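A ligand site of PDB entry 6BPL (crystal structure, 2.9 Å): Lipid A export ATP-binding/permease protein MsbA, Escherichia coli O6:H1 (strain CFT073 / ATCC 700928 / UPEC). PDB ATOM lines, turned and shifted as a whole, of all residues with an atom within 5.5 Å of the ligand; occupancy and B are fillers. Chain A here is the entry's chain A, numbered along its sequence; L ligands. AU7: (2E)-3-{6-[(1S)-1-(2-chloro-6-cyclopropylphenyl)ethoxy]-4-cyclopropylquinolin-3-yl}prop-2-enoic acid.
The guanidinium group (NH2) of Arg 190 is in salt-bridge range of an oxygen (O28) of the ligand, at 2.9 Å.
An oxygen (O28) of the ligand lies within salt-bridge range of the side-chain amino group (NZ) of Lys 299, 3.8 Å away.
Phe 157 touches the ligand (CZ to C12, 3.3 Å).
Leu 171 touches the ligand.
Ala 175 touches the ligand.
Val 178 touches the ligand (CG1 to C19, 3.8 Å).
Ser 179 touches the ligand (OG to C16, 3.0 Å).
CD1 of Ile 182 touches C20 of the ligand (3.4 Å).
CG2 of Ile 255 touches C26 of the ligand, at 3.9 Å.
O of Ala 259 touches CL9 of the ligand, at 3.4 Å.
Ala 262 touches the ligand (CB to C1, 3.9 Å).
Leu 263 touches the ligand (CG to CL9, 3.96 Å).
Met 291 touches the ligand.
Leu 294 touches the ligand (CB to C6, 3.5 Å).
Met 295 touches the ligand (CG to C30, 3.6 Å).
Leu 298 touches the ligand.
Hydrophobic or aromatic side chains that line the ligand: Phe 157, Leu 171, Ala 175, Val 178, Ile 182, Ile 255, Ala 259, Ala 262, Leu 263, Leu 294, Met 295 and Leu 298.
16 residues have an atom within 4 Å of the ligand: Phe 157, Leu 171, Ala 175, Val 178, Ser 179, Ile 182, Arg 190, Ile 255, Ala 259, Ala 262, Leu 263, Met 291, Leu 294, Met 295, Leu 298 and Lys 299.
The nearest printed residue that does not touch the ligand is Ile 172 (4.2 Å).
The backbone carbonyl oxygen (O) of Ala 175 is in hydrogen-bond range of the side-chain hydroxyl (OG) of Ser 179, 2.7 Å away.
OG1 of Thr 302 lies within hydrogen-bond range of O of Lys 299.
O of Lys 299 sits close to OD1 of Asn 303.
The side-chain hydroxyl of Thr 302 sits at hydrogen-bond distance from the backbone carbonyl oxygen of Leu 298.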
ATOM      1  N   PHE A 157       6.395  13.959  10.547  1.00  0.00           N
ATOM      2  CA  PHE A 157       5.742  13.964   9.243  1.00  0.00           C
ATOM      3  C   PHE A 157       5.002  12.664   8.993  1.00  0.00           C
ATOM      4  O   PHE A 157       3.869  12.668   8.496  1.00  0.00           O
ATOM      5  CB  PHE A 157       6.780  14.180   8.135  1.00  0.00           C
ATOM      6  CG  PHE A 157       6.826  15.594   7.614  1.00  0.00           C
ATOM      7  CD1 PHE A 157       5.658  16.308   7.379  1.00  0.00           C
ATOM      8  CD2 PHE A 157       8.040  16.211   7.330  1.00  0.00           C
ATOM      9  CE1 PHE A 157       5.704  17.601   6.901  1.00  0.00           C
ATOM     10  CE2 PHE A 157       8.085  17.494   6.838  1.00  0.00           C
ATOM     11  CZ  PHE A 157       6.914  18.191   6.630  1.00  0.00           C
ATOM     12  N   LEU A 171      -1.029  21.176   4.908  1.00  0.00           N
ATOM     13  CA  LEU A 171       0.134  21.812   5.488  1.00  0.00           C
ATOM     14  C   LEU A 171       1.286  21.867   4.492  1.00  0.00           C
ATOM     15  O   LEU A 171       1.997  22.868   4.396  1.00  0.00           O
ATOM     16  CB  LEU A 171       0.564  21.056   6.754  1.00  0.00           C
ATOM     17  CG  LEU A 171       1.320  21.860   7.808  1.00  0.00           C
ATOM     18  CD1 LEU A 171       0.414  22.878   8.472  1.00  0.00           C
ATOM     19  CD2 LEU A 171       1.892  20.909   8.842  1.00  0.00           C
ATOM     20  N   ILE A 172       1.470  20.795   3.714  1.00  0.00           N
ATOM     21  CA  ILE A 172       2.612  20.711   2.809  1.00  0.00           C
ATOM     22  C   ILE A 172       2.442  21.697   1.661  1.00  0.00           C
ATOM     23  O   ILE A 172       3.385  22.428   1.307  1.00  0.00           O
ATOM     24  CB  ILE A 172       2.776  19.271   2.299  1.00  0.00           C
ATOM     25  CG1 ILE A 172       3.624  18.464   3.290  1.00  0.00           C
ATOM     26  CG2 ILE A 172       3.423  19.237   0.920  1.00  0.00           C
ATOM     27  CD1 ILE A 172       2.987  18.285   4.657  1.00  0.00           C
ATOM     28  N   LEU A 174       0.888  24.394   1.682  1.00  0.00           N
ATOM     29  CA  LEU A 174       1.138  25.715   2.257  1.00  0.00           C
ATOM     30  C   LEU A 174       2.610  25.927   2.582  1.00  0.00           C
ATOM     31  O   LEU A 174       3.040  27.085   2.719  1.00  0.00           O
ATOM     32  CB  LEU A 174       0.299  25.897   3.526  1.00  0.00           C
ATOM     33  CG  LEU A 174      -1.085  26.542   3.365  1.00  0.00           C
ATOM     34  CD1 LEU A 174      -1.868  26.431   4.664  1.00  0.00           C
ATOM     35  CD2 LEU A 174      -0.949  27.997   2.955  1.00  0.00           C
ATOM     36  N   ALA A 175       3.399  24.864   2.680  1.00  0.00           N
ATOM     37  CA  ALA A 175       4.770  24.986   3.176  1.00  0.00           C
ATOM     38  C   ALA A 175       5.609  25.957   2.364  1.00  0.00           C
ATOM     39  O   ALA A 175       6.208  26.870   2.962  1.00  0.00           O
ATOM     40  CB  ALA A 175       5.427  23.601   3.229  1.00  0.00           C
ATOM     41  N   VAL A 178       4.658  29.685   2.885  1.00  0.00           N
ATOM     42  CA  VAL A 178       4.949  30.000   4.286  1.00  0.00           C
ATOM     43  C   VAL A 178       6.457  30.102   4.483  1.00  0.00           C
ATOM     44  O   VAL A 178       6.950  31.005   5.174  1.00  0.00           O
ATOM     45  CB  VAL A 178       4.318  28.960   5.222  1.00  0.00           C
ATOM     46  CG1 VAL A 178       4.786  29.159   6.659  1.00  0.00           C
ATOM     47  CG2 VAL A 178       2.797  29.034   5.141  1.00  0.00           C
ATOM     48  N   SER A 179       7.211  29.178   3.889  1.00  0.00           N
ATOM     49  CA  SER A 179       8.665  29.229   3.989  1.00  0.00           C
ATOM     50  C   SER A 179       9.200  30.541   3.413  1.00  0.00           C
ATOM     51  O   SER A 179       9.956  31.256   4.063  1.00  0.00           O
ATOM     52  CB  SER A 179       9.283  28.036   3.261  1.00  0.00           C
ATOM     53  OG  SER A 179       8.778  26.823   3.773  1.00  0.00           O
ATOM     54  N   ILE A 182       8.423  33.449   5.503  1.00  0.00           N
ATOM     55  CA  ILE A 182       9.238  33.542   6.706  1.00  0.00           C
ATOM     56  C   ILE A 182      10.653  34.002   6.368  1.00  0.00           C
ATOM     57  O   ILE A 182      11.223  34.848   7.063  1.00  0.00           O
ATOM     58  CB  ILE A 182       9.224  32.193   7.449  1.00  0.00           C
ATOM     59  CG1 ILE A 182       7.822  31.908   7.975  1.00  0.00           C
ATOM     60  CG2 ILE A 182      10.234  32.193   8.589  1.00  0.00           C
ATOM     61  CD1 ILE A 182       7.609  30.479   8.445  1.00  0.00           C
ATOM     62  N   ARG A 190      16.609  40.685  10.716  1.00  0.00           N
ATOM     63  CA  ARG A 190      17.613  40.152  11.638  1.00  0.00           C
ATOM     64  C   ARG A 190      18.830  39.650  10.866  1.00  0.00           C
ATOM     65  O   ARG A 190      18.905  38.500  10.456  1.00  0.00           O
ATOM     66  CB  ARG A 190      17.004  39.053  12.510  1.00  0.00           C
ATOM     67  CG  ARG A 190      16.225  37.965  11.784  1.00  0.00           C
ATOM     68  CD  ARG A 190      15.329  37.246  12.786  1.00  0.00           C
ATOM     69  NE  ARG A 190      14.726  36.029  12.263  1.00  0.00           N
ATOM     70  CZ  ARG A 190      13.921  35.235  12.964  1.00  0.00           C
ATOM     71  NH1 ARG A 190      13.627  35.527  14.226  1.00  0.00           N
ATOM     72  NH2 ARG A 190      13.420  34.137  12.419  1.00  0.00           N
ATOM     73  N   ILE A 255       6.751  36.168  12.359  1.00  0.00           N
ATOM     74  CA  ILE A 255       6.985  34.876  11.722  1.00  0.00           C
ATOM     75  C   ILE A 255       5.995  33.833  12.226  1.00  0.00           C
ATOM     76  O   ILE A 255       5.379  33.106  11.440  1.00  0.00           O
ATOM     77  CB  ILE A 255       8.447  34.438  11.927  1.00  0.00           C
ATOM     78  CG1 ILE A 255       9.347  35.224  10.968  1.00  0.00           C
ATOM     79  CG2 ILE A 255       8.603  32.930  11.712  1.00  0.00           C
ATOM     80  CD1 ILE A 255      10.819  34.978  11.144  1.00  0.00           C
ATOM     81  N   ALA A 259       3.067  31.510  10.367  1.00  0.00           N
ATOM     82  CA  ALA A 259       2.801  30.091  10.611  1.00  0.00           C
ATOM     83  C   ALA A 259       1.487  29.876  11.355  1.00  0.00           C
ATOM     84  O   ALA A 259       0.962  28.764  11.329  1.00  0.00           O
ATOM     85  CB  ALA A 259       3.951  29.485  11.407  1.00  0.00           C
ATOM     86  N   SER A 260       0.956  30.913  12.008  1.00  0.00           N
ATOM     87  CA  SER A 260      -0.329  30.787  12.673  1.00  0.00           C
ATOM     88  C   SER A 260      -1.472  30.783  11.652  1.00  0.00           C
ATOM     89  O   SER A 260      -2.458  30.069  11.824  1.00  0.00           O
ATOM     90  CB  SER A 260      -0.515  31.916  13.673  1.00  0.00           C
ATOM     91  OG  SER A 260      -1.711  31.744  14.420  1.00  0.00           O
ATOM     92  N   ALA A 262      -1.213  29.583   8.500  1.00  0.00           N
ATOM     93  CA  ALA A 262      -1.184  28.303   7.793  1.00  0.00           C
ATOM     94  C   ALA A 262      -1.846  27.197   8.614  1.00  0.00           C
ATOM     95  O   ALA A 262      -2.406  26.257   8.035  1.00  0.00           O
ATOM     96  CB  ALA A 262       0.254  27.929   7.458  1.00  0.00           C
ATOM     97  N   LEU A 263      -1.782  27.269   9.942  1.00  0.00           N
ATOM     98  CA  LEU A 263      -2.393  26.237  10.773  1.00  0.00           C
ATOM     99  C   LEU A 263      -3.896  26.459  10.912  1.00  0.00           C
ATOM    100  O   LEU A 263      -4.656  25.487  10.960  1.00  0.00           O
ATOM    101  CB  LEU A 263      -1.746  26.204  12.153  1.00  0.00           C
ATOM    102  CG  LEU A 263      -0.336  25.619  12.258  1.00  0.00           C
ATOM    103  CD1 LEU A 263       0.113  25.626  13.704  1.00  0.00           C
ATOM    104  CD2 LEU A 263      -0.250  24.209  11.692  1.00  0.00           C
ATOM    105  N   MET A 291       1.927  18.908  14.355  1.00  0.00           N
ATOM    106  CA  MET A 291       2.214  20.112  13.576  1.00  0.00           C
ATOM    107  C   MET A 291       2.842  21.187  14.462  1.00  0.00           C
ATOM    108  O   MET A 291       3.786  21.861  14.056  1.00  0.00           O
ATOM    109  CB  MET A 291       0.939  20.631  12.922  1.00  0.00           C
ATOM    110  CG  MET A 291       0.308  19.666  11.937  1.00  0.00           C
ATOM    111  SD  MET A 291      -1.217  20.307  11.214  1.00  0.00           S
ATOM    112  CE  MET A 291      -1.553  19.071   9.964  1.00  0.00           C
ATOM    113  N   ILE A 292       2.321  21.353  15.682  1.00  0.00           N
ATOM    114  CA  ILE A 292       2.915  22.294  16.620  1.00  0.00           C
ATOM    115  C   ILE A 292       4.325  21.839  16.973  1.00  0.00           C
ATOM    116  O   ILE A 292       5.269  22.639  16.995  1.00  0.00           O
ATOM    117  CB  ILE A 292       2.035  22.436  17.869  1.00  0.00           C
ATOM    118  CG1 ILE A 292       0.767  23.228  17.523  1.00  0.00           C
ATOM    119  CG2 ILE A 292       2.795  23.116  19.018  1.00  0.00           C
ATOM    120  CD1 ILE A 292      -0.239  23.336  18.657  1.00  0.00           C
ATOM    121  N   LEU A 294       6.261  20.374  15.182  1.00  0.00           N
ATOM    122  CA  LEU A 294       7.125  20.568  14.021  1.00  0.00           C
ATOM    123  C   LEU A 294       7.727  21.962  13.967  1.00  0.00           C
ATOM    124  O   LEU A 294       8.717  22.162  13.252  1.00  0.00           O
ATOM    125  CB  LEU A 294       6.346  20.315  12.725  1.00  0.00           C
ATOM    126  CG  LEU A 294       6.286  18.910  12.122  1.00  0.00           C
ATOM    127  CD1 LEU A 294       5.588  18.985  10.763  1.00  0.00           C
ATOM    128  CD2 LEU A 294       7.666  18.292  11.974  1.00  0.00           C
ATOM    129  N   MET A 295       7.165  22.925  14.693  1.00  0.00           N
ATOM    130  CA  MET A 295       7.574  24.306  14.516  1.00  0.00           C
ATOM    131  C   MET A 295       9.002  24.527  15.019  1.00  0.00           C
ATOM    132  O   MET A 295       9.782  25.234  14.366  1.00  0.00           O
ATOM    133  CB  MET A 295       6.601  25.234  15.231  1.00  0.00           C
ATOM    134  CG  MET A 295       5.225  25.288  14.595  1.00  0.00           C
ATOM    135  SD  MET A 295       4.166  26.598  15.260  1.00  0.00           S
ATOM    136  CE  MET A 295       3.886  26.003  16.923  1.00  0.00           C
ATOM    137  N   ARG A 296       9.350  23.957  16.168  1.00  0.00           N
ATOM    138  CA  ARG A 296      10.695  24.165  16.696  1.00  0.00           C
ATOM    139  C   ARG A 296      11.746  23.511  15.814  1.00  0.00           C
ATOM    140  O   ARG A 296      12.720  24.181  15.425  1.00  0.00           O
ATOM    141  CB  ARG A 296      10.782  23.663  18.140  1.00  0.00           C
ATOM    142  CG  ARG A 296      12.137  23.880  18.809  1.00  0.00           C
ATOM    143  CD  ARG A 296      12.467  25.364  18.943  1.00  0.00           C
ATOM    144  NE  ARG A 296      11.523  26.039  19.842  1.00  0.00           N
ATOM    145  CZ  ARG A 296      11.555  27.329  20.131  1.00  0.00           C
ATOM    146  NH1 ARG A 296      12.479  28.123  19.599  1.00  0.00           N
ATOM    147  NH2 ARG A 296      10.646  27.841  20.948  1.00  0.00           N
ATOM    148  N   LEU A 298      11.726  22.847  12.591  1.00  0.00           N
ATOM    149  CA  LEU A 298      11.866  23.626  11.359  1.00  0.00           C
ATOM    150  C   LEU A 298      12.628  24.921  11.605  1.00  0.00           C
ATOM    151  O   LEU A 298      13.353  25.394  10.715  1.00  0.00           O
ATOM    152  CB  LEU A 298      10.494  23.928  10.767  1.00  0.00           C
ATOM    153  CG  LEU A 298       9.671  22.735  10.286  1.00  0.00           C
ATOM    154  CD1 LEU A 298       8.278  23.199   9.892  1.00  0.00           C
ATOM    155  CD2 LEU A 298      10.343  22.030   9.128  1.00  0.00           C
ATOM    156  N   LYS A 299      12.471  25.523  12.780  1.00  0.00           N
ATOM    157  CA  LYS A 299      13.231  26.731  13.102  1.00  0.00           C
ATOM    158  C   LYS A 299      14.710  26.409  13.282  1.00  0.00           C
ATOM    159  O   LYS A 299      15.571  27.140  12.788  1.00  0.00           O
ATOM    160  CB  LYS A 299      12.672  27.376  14.366  1.00  0.00           C
ATOM    161  CG  LYS A 299      13.597  28.413  14.984  1.00  0.00           C
ATOM    162  CD  LYS A 299      12.906  29.207  16.080  1.00  0.00           C
ATOM    163  CE  LYS A 299      13.818  30.280  16.659  1.00  0.00           C
ATOM    164  NZ  LYS A 299      14.290  31.247  15.606  1.00  0.00           N
ATOM    165  N   THR A 302      16.629  25.397   9.607  1.00  0.00           N
ATOM    166  CA  THR A 302      16.901  26.457   8.640  1.00  0.00           C
ATOM    167  C   THR A 302      17.927  27.457   9.149  1.00  0.00           C
ATOM    168  O   THR A 302      18.320  28.343   8.375  1.00  0.00           O
ATOM    169  CB  THR A 302      15.608  27.194   8.278  1.00  0.00           C
ATOM    170  OG1 THR A 302      14.914  27.596   9.460  1.00  0.00           O
ATOM    171  CG2 THR A 302      14.708  26.306   7.412  1.00  0.00           C
ATOM    172  N   ASN A 303      18.378  27.348  10.395  1.00  0.00           N
ATOM    173  CA  ASN A 303      19.449  28.191  10.929  1.00  0.00           C
ATOM    174  C   ASN A 303      20.741  27.411  11.139  1.00  0.00           C
ATOM    175  O   ASN A 303      21.618  27.868  11.878  1.00  0.00           O
ATOM    176  CB  ASN A 303      19.000  28.834  12.235  1.00  0.00           C
ATOM    177  CG  ASN A 303      17.761  29.692  12.069  1.00  0.00           C
ATOM    178  OD1 ASN A 303      16.768  29.521  12.783  1.00  0.00           O
ATOM    179  ND2 ASN A 303      17.796  30.608  11.108  1.00  0.00           N
HETATM  180  C4  AU7 L   1       4.863  23.168   8.630  1.00  0.00           C
HETATM  181  C14 AU7 L   1       6.538  25.825   7.235  1.00  0.00           C
HETATM  182  C5  AU7 L   1       4.941  22.275   9.694  1.00  0.00           C
HETATM  183  C6  AU7 L   1       4.414  22.607  10.930  1.00  0.00           C
HETATM  184  C11 AU7 L   1       4.657  21.725   6.486  1.00  0.00           C
HETATM  185  C7  AU7 L   1       3.823  23.844  11.116  1.00  0.00           C
HETATM  186  C8  AU7 L   1       3.760  24.739  10.052  1.00  0.00           C
HETATM  187  C10 AU7 L   1       5.440  22.760   7.298  1.00  0.00           C
HETATM  188  C12 AU7 L   1       5.972  21.330   7.157  1.00  0.00           C
HETATM  189  C3  AU7 L   1       4.273  24.405   8.817  1.00  0.00           C
HETATM  190  C1  AU7 L   1       2.916  25.174   6.875  1.00  0.00           C
HETATM  191  C15 AU7 L   1       7.600  25.617   6.349  1.00  0.00           C
HETATM  192  C16 AU7 L   1       8.861  26.019   6.634  1.00  0.00           C
HETATM  193  C17 AU7 L   1       9.121  26.686   7.842  1.00  0.00           C
HETATM  194  C18 AU7 L   1       8.060  26.914   8.756  1.00  0.00           C
HETATM  195  C19 AU7 L   1       6.764  26.473   8.429  1.00  0.00           C
HETATM  196  C2  AU7 L   1       4.173  25.427   7.705  1.00  0.00           C
HETATM  197  C20 AU7 L   1       8.349  27.581   9.971  1.00  0.00           C
HETATM  198  C21 AU7 L   1       9.677  27.978  10.195  1.00  0.00           C
HETATM  199  C22 AU7 L   1      10.659  27.714   9.223  1.00  0.00           C
HETATM  200  C24 AU7 L   1      10.096  28.706  11.407  1.00  0.00           C
HETATM  201  C25 AU7 L   1      11.058  29.642  11.262  1.00  0.00           C
HETATM  202  C26 AU7 L   1      11.551  30.434  12.392  1.00  0.00           C
HETATM  203  C29 AU7 L   1       7.269  27.867  10.993  1.00  0.00           C
HETATM  204  C30 AU7 L   1       6.549  26.662  11.595  1.00  0.00           C
HETATM  205  C31 AU7 L   1       7.525  27.483  12.451  1.00  0.00           C
HETATM  206  N23 AU7 L   1      10.367  27.090   8.119  1.00  0.00           N
HETATM  207  O13 AU7 L   1       5.315  25.377   6.833  1.00  0.00           O
HETATM  208  O27 AU7 L   1      11.085  30.273  13.503  1.00  0.00           O
HETATM  209  O28 AU7 L   1      12.517  31.363  12.202  1.00  0.00           O
HETATM  210 CL9  AU7 L   1       3.024  26.281  10.265  1.00  0.00          CL
